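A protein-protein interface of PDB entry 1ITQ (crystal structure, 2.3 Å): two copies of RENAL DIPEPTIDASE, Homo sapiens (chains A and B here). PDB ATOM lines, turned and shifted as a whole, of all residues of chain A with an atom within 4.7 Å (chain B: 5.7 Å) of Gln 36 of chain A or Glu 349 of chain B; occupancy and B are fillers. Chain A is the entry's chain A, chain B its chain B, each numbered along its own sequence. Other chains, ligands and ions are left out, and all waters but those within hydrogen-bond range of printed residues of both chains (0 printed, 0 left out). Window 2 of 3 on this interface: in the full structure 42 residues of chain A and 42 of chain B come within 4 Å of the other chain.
OE1 of Glu 349 of chain B is in hydrogen-bond range of N of Leu 35 of chain A, at 3.1 Å. The backbone NH (N) of Gln 36 of chain A sits at hydrogen-bond distance from the side-chain carboxylate (OE1) of Glu 349 of chain B, 2.9 Å away. NH2 of Arg 91 of chain A is in salt-bridge range of OE2 of Glu 349 of chain B (2.9 Å).
O of Glu 348 of chain B lies within hydrogen-bond range of NH2 of Arg 138 of chain B (2.7 Å). NH1 of Arg 91 of chain A lies within hydrogen-bond range of O of Asn 33 of chain A, at 2.9 Å.
Asn 33 of chain A touches Glu 349 of chain B (O to OE2, 3.97 Å). Arg 34 of chain A touches Glu 349 of chain B (C to OE1, 3.1 Å). Arg 34 of chain A touches Glu 350 of chain B. CB of Ala 346 of chain B touches OE1 of Gln 36 of chain A, at 3.7 Å. NH1 of Arg 138 of chain B touches NE of Arg 91 of chain A, 3.7 Å away. CD of Arg 91 of chain A touches CB of Pro 347 of chain B, at 3.9 Å.
Of the printed residues of chain B, Gln 36 of chain A touches Ala 346 and Glu 349. Glu 349 of chain B touches just these residues of chain A: Asn 33, Arg 34, Leu 35, Gln 36 and Arg 91. Of the printed residues of chain B, Arg 91 of chain A touches Arg 138 (3.7 Å), Pro 347 (3.9 Å) and Glu 349 (2.9 Å). Of the printed residues of chain A, Arg 138 of chain B touches Arg 91. Of the printed residues of chain B, Leu 35 of chain A touches Glu 349. Printed residues of chain A within 4 Å of Pro 347 of chain B: Arg 91. Glu 348 of chain B touches none of the printed residues of chain A. The nearest residue of chain B that does not touch Gln 36 of chain A is Pro 347 of chain B (4.2 Å).
Hydrophobic or aromatic side chains of chain A that line the printed part of chain B: Leu 35. Printed residues of chain B that touch a printed residue of chain A: Arg 138, Ala 346, Pro 347, Glu 349 and Glu 350. Hydrophobic or aromatic side chains of chain B within 4 Å of the printed part of chain A: Ala 346 and Pro 347.
No position is printed for both chains.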
ATOM      1  N   ASN A  33     -18.441 -26.280  17.983  1.00  0.00           N
ATOM      2  CA  ASN A  33     -17.822 -27.504  17.494  1.00  0.00           C
ATOM      3  C   ASN A  33     -17.265 -27.463  16.073  1.00  0.00           C
ATOM      4  O   ASN A  33     -16.952 -28.506  15.493  1.00  0.00           O
ATOM      5  CB  ASN A  33     -18.774 -28.695  17.672  1.00  0.00           C
ATOM      6  CG  ASN A  33     -18.944 -29.100  19.134  1.00  0.00           C
ATOM      7  OD1 ASN A  33     -17.985 -29.088  19.906  1.00  0.00           O
ATOM      8  ND2 ASN A  33     -20.162 -29.476  19.511  1.00  0.00           N
ATOM      9  N   ARG A  34     -17.107 -26.261  15.526  1.00  0.00           N
ATOM     10  CA  ARG A  34     -16.551 -26.102  14.181  1.00  0.00           C
ATOM     11  C   ARG A  34     -15.022 -26.109  14.257  1.00  0.00           C
ATOM     12  O   ARG A  34     -14.393 -25.064  14.350  1.00  0.00           O
ATOM     13  CB  ARG A  34     -17.063 -24.811  13.540  1.00  0.00           C
ATOM     14  CG  ARG A  34     -18.568 -24.784  13.354  1.00  0.00           C
ATOM     15  CD  ARG A  34     -19.040 -23.439  12.851  1.00  0.00           C
ATOM     16  NE  ARG A  34     -18.533 -23.164  11.511  1.00  0.00           N
ATOM     17  CZ  ARG A  34     -19.261 -22.647  10.524  1.00  0.00           C
ATOM     18  NH1 ARG A  34     -18.712 -22.438   9.331  1.00  0.00           N
ATOM     19  NH2 ARG A  34     -20.538 -22.333  10.727  1.00  0.00           N
ATOM     20  N   LEU A  35     -14.444 -27.305  14.201  1.00  0.00           N
ATOM     21  CA  LEU A  35     -13.001 -27.512  14.288  1.00  0.00           C
ATOM     22  C   LEU A  35     -12.141 -26.974  13.145  1.00  0.00           C
ATOM     23  O   LEU A  35     -10.911 -26.905  13.273  1.00  0.00           O
ATOM     24  CB  LEU A  35     -12.696 -29.001  14.464  1.00  0.00           C
ATOM     25  CG  LEU A  35     -13.236 -29.723  15.700  1.00  0.00           C
ATOM     26  CD1 LEU A  35     -12.683 -31.126  15.676  1.00  0.00           C
ATOM     27  CD2 LEU A  35     -12.833 -29.012  16.986  1.00  0.00           C
ATOM     28  N   GLN A  36     -12.764 -26.667  12.009  1.00  0.00           N
ATOM     29  CA  GLN A  36     -12.025 -26.139  10.862  1.00  0.00           C
ATOM     30  C   GLN A  36     -11.880 -24.630  10.929  1.00  0.00           C
ATOM     31  O   GLN A  36     -11.199 -24.028  10.104  1.00  0.00           O
ATOM     32  CB  GLN A  36     -12.663 -26.569   9.544  1.00  0.00           C
ATOM     33  CG  GLN A  36     -12.494 -28.046   9.268  1.00  0.00           C
ATOM     34  CD  GLN A  36     -12.933 -28.429   7.881  1.00  0.00           C
ATOM     35  OE1 GLN A  36     -12.106 -28.592   6.981  1.00  0.00           O
ATOM     36  NE2 GLN A  36     -14.240 -28.579   7.692  1.00  0.00           N
ATOM     37  N   ASP A  37     -12.538 -24.033  11.918  1.00  0.00           N
ATOM     38  CA  ASP A  37     -12.466 -22.601  12.163  1.00  0.00           C
ATOM     39  C   ASP A  37     -11.010 -22.362  12.567  1.00  0.00           C
ATOM     40  O   ASP A  37     -10.431 -23.141  13.329  1.00  0.00           O
ATOM     41  CB  ASP A  37     -13.404 -22.236  13.316  1.00  0.00           C
ATOM     42  CG  ASP A  37     -13.563 -20.741  13.497  1.00  0.00           C
ATOM     43  OD1 ASP A  37     -12.546 -20.036  13.678  1.00  0.00           O
ATOM     44  OD2 ASP A  37     -14.721 -20.272  13.477  1.00  0.00           O
ATOM     45  N   GLU A  38     -10.411 -21.307  12.026  1.00  0.00           N
ATOM     46  CA  GLU A  38      -9.010 -20.986  12.304  1.00  0.00           C
ATOM     47  C   GLU A  38      -8.647 -20.723  13.773  1.00  0.00           C
ATOM     48  O   GLU A  38      -7.597 -21.176  14.245  1.00  0.00           O
ATOM     49  CB  GLU A  38      -8.536 -19.848  11.388  1.00  0.00           C
ATOM     50  CG  GLU A  38      -9.585 -18.772  11.102  1.00  0.00           C
ATOM     51  CD  GLU A  38      -9.260 -17.955   9.858  1.00  0.00           C
ATOM     52  OE1 GLU A  38      -9.743 -18.323   8.760  1.00  0.00           O
ATOM     53  OE2 GLU A  38      -8.522 -16.949   9.973  1.00  0.00           O
ATOM     54  N   ARG A  91     -13.717 -36.489  16.267  1.00  0.00           N
ATOM     55  CA  ARG A  91     -13.174 -35.661  15.191  1.00  0.00           C
ATOM     56  C   ARG A  91     -11.834 -35.039  15.528  1.00  0.00           C
ATOM     57  O   ARG A  91     -10.941 -34.967  14.683  1.00  0.00           O
ATOM     58  CB  ARG A  91     -14.183 -34.585  14.796  1.00  0.00           C
ATOM     59  CG  ARG A  91     -15.399 -35.163  14.097  1.00  0.00           C
ATOM     60  CD  ARG A  91     -16.203 -34.119  13.376  1.00  0.00           C
ATOM     61  NE  ARG A  91     -16.992 -33.279  14.262  1.00  0.00           N
ATOM     62  CZ  ARG A  91     -16.893 -31.956  14.300  1.00  0.00           C
ATOM     63  NH1 ARG A  91     -17.663 -31.262  15.120  1.00  0.00           N
ATOM     64  NH2 ARG A  91     -15.995 -31.335  13.544  1.00  0.00           N
ATOM     65  N   MET A  95      -8.451 -35.234  13.282  1.00  0.00           N
ATOM     66  CA  MET A  95      -7.863 -34.018  12.744  1.00  0.00           C
ATOM     67  C   MET A  95      -6.411 -33.866  13.218  1.00  0.00           C
ATOM     68  O   MET A  95      -5.567 -33.355  12.477  1.00  0.00           O
ATOM     69  CB  MET A  95      -8.709 -32.818  13.166  1.00  0.00           C
ATOM     70  CG  MET A  95      -8.399 -31.544  12.430  1.00  0.00           C
ATOM     71  SD  MET A  95      -9.751 -30.396  12.621  1.00  0.00           S
ATOM     72  CE  MET A  95     -10.888 -31.008  11.334  1.00  0.00           C
ATOM     73  N   LEU B 134     -25.546 -32.959  12.379  1.00  0.00           N
ATOM     74  CA  LEU B 134     -24.573 -33.704  11.607  1.00  0.00           C
ATOM     75  C   LEU B 134     -23.812 -34.607  12.558  1.00  0.00           C
ATOM     76  O   LEU B 134     -23.359 -35.675  12.165  1.00  0.00           O
ATOM     77  CB  LEU B 134     -23.637 -32.735  10.884  1.00  0.00           C
ATOM     78  CG  LEU B 134     -24.314 -31.918   9.780  1.00  0.00           C
ATOM     79  CD1 LEU B 134     -23.393 -30.819   9.288  1.00  0.00           C
ATOM     80  CD2 LEU B 134     -24.711 -32.841   8.635  1.00  0.00           C
ATOM     81  N   ARG B 138     -23.478 -38.698  12.375  1.00  0.00           N
ATOM     82  CA  ARG B 138     -22.260 -39.512  12.424  1.00  0.00           C
ATOM     83  C   ARG B 138     -22.302 -40.539  13.552  1.00  0.00           C
ATOM     84  O   ARG B 138     -21.684 -41.597  13.448  1.00  0.00           O
ATOM     85  CB  ARG B 138     -21.009 -38.631  12.569  1.00  0.00           C
ATOM     86  CG  ARG B 138     -20.542 -37.961  11.282  1.00  0.00           C
ATOM     87  CD  ARG B 138     -19.341 -37.066  11.538  1.00  0.00           C
ATOM     88  NE  ARG B 138     -19.677 -35.860  12.300  1.00  0.00           N
ATOM     89  CZ  ARG B 138     -19.974 -34.675  11.765  1.00  0.00           C
ATOM     90  NH1 ARG B 138     -20.254 -33.636  12.543  1.00  0.00           N
ATOM     91  NH2 ARG B 138     -20.010 -34.526  10.448  1.00  0.00           N
ATOM     92  N   ALA B 346     -13.013 -34.230   5.158  1.00  0.00           N
ATOM     93  CA  ALA B 346     -13.444 -33.581   6.386  1.00  0.00           C
ATOM     94  C   ALA B 346     -14.953 -33.617   6.565  1.00  0.00           C
ATOM     95  O   ALA B 346     -15.701 -33.243   5.660  1.00  0.00           O
ATOM     96  CB  ALA B 346     -12.953 -32.145   6.411  1.00  0.00           C
ATOM     97  N   PRO B 347     -15.417 -34.064   7.747  1.00  0.00           N
ATOM     98  CA  PRO B 347     -16.836 -34.158   8.087  1.00  0.00           C
ATOM     99  C   PRO B 347     -17.499 -32.797   7.996  1.00  0.00           C
ATOM    100  O   PRO B 347     -16.851 -31.777   8.204  1.00  0.00           O
ATOM    101  CB  PRO B 347     -16.799 -34.628   9.541  1.00  0.00           C
ATOM    102  CG  PRO B 347     -15.578 -35.455   9.596  1.00  0.00           C
ATOM    103  CD  PRO B 347     -14.594 -34.598   8.844  1.00  0.00           C
ATOM    104  N   GLU B 348     -18.777 -32.777   7.644  1.00  0.00           N
ATOM    105  CA  GLU B 348     -19.510 -31.521   7.578  1.00  0.00           C
ATOM    106  C   GLU B 348     -19.729 -31.076   9.021  1.00  0.00           C
ATOM    107  O   GLU B 348     -20.071 -31.888   9.886  1.00  0.00           O
ATOM    108  CB  GLU B 348     -20.856 -31.706   6.868  1.00  0.00           C
ATOM    109  CG  GLU B 348     -20.769 -31.824   5.354  1.00  0.00           C
ATOM    110  CD  GLU B 348     -20.276 -30.547   4.705  1.00  0.00           C
ATOM    111  OE1 GLU B 348     -20.797 -29.451   5.023  1.00  0.00           O
ATOM    112  OE2 GLU B 348     -19.346 -30.644   3.882  1.00  0.00           O
ATOM    113  N   GLU B 349     -19.541 -29.787   9.278  1.00  0.00           N
ATOM    114  CA  GLU B 349     -19.699 -29.267  10.626  1.00  0.00           C
ATOM    115  C   GLU B 349     -20.445 -27.946  10.727  1.00  0.00           C
ATOM    116  O   GLU B 349     -20.573 -27.400  11.821  1.00  0.00           O
ATOM    117  CB  GLU B 349     -18.336 -29.150  11.305  1.00  0.00           C
ATOM    118  CG  GLU B 349     -17.366 -28.259  10.563  1.00  0.00           C
ATOM    119  CD  GLU B 349     -16.060 -28.073  11.297  1.00  0.00           C
ATOM    120  OE1 GLU B 349     -15.568 -26.927  11.333  1.00  0.00           O
ATOM    121  OE2 GLU B 349     -15.523 -29.067  11.828  1.00  0.00           O
ATOM    122  N   GLU B 350     -20.920 -27.421   9.601  1.00  0.00           N
ATOM    123  CA  GLU B 350     -21.676 -26.171   9.629  1.00  0.00           C
ATOM    124  C   GLU B 350     -23.088 -26.517  10.117  1.00  0.00           C
ATOM    125  O   GLU B 350     -23.886 -27.113   9.393  1.00  0.00           O
ATOM    126  CB  GLU B 350     -21.712 -25.532   8.239  1.00  0.00           C
ATOM    127  CG  GLU B 350     -22.325 -24.125   8.195  1.00  0.00           C
ATOM    128  CD  GLU B 350     -22.417 -23.545   6.773  1.00  0.00           C
ATOM    129  OE1 GLU B 350     -23.223 -22.607   6.568  1.00  0.00           O
ATOM    130  OE2 GLU B 350     -21.692 -24.023   5.864  1.00  0.00           O
ATOM    131  N   PRO B 351     -23.401 -26.173  11.373  1.00  0.00           N
ATOM    132  CA  PRO B 351     -24.720 -26.471  11.926  1.00  0.00           C
ATOM    133  C   PRO B 351     -25.883 -25.786  11.221  1.00  0.00           C
ATOM    134  O   PRO B 351     -25.707 -24.851  10.439  1.00  0.00           O
ATOM    135  CB  PRO B 351     -24.588 -25.997  13.369  1.00  0.00           C
ATOM    136  CG  PRO B 351     -23.685 -24.831  13.236  1.00  0.00           C
ATOM    137  CD  PRO B 351     -22.611 -25.380  12.328  1.00  0.00           C
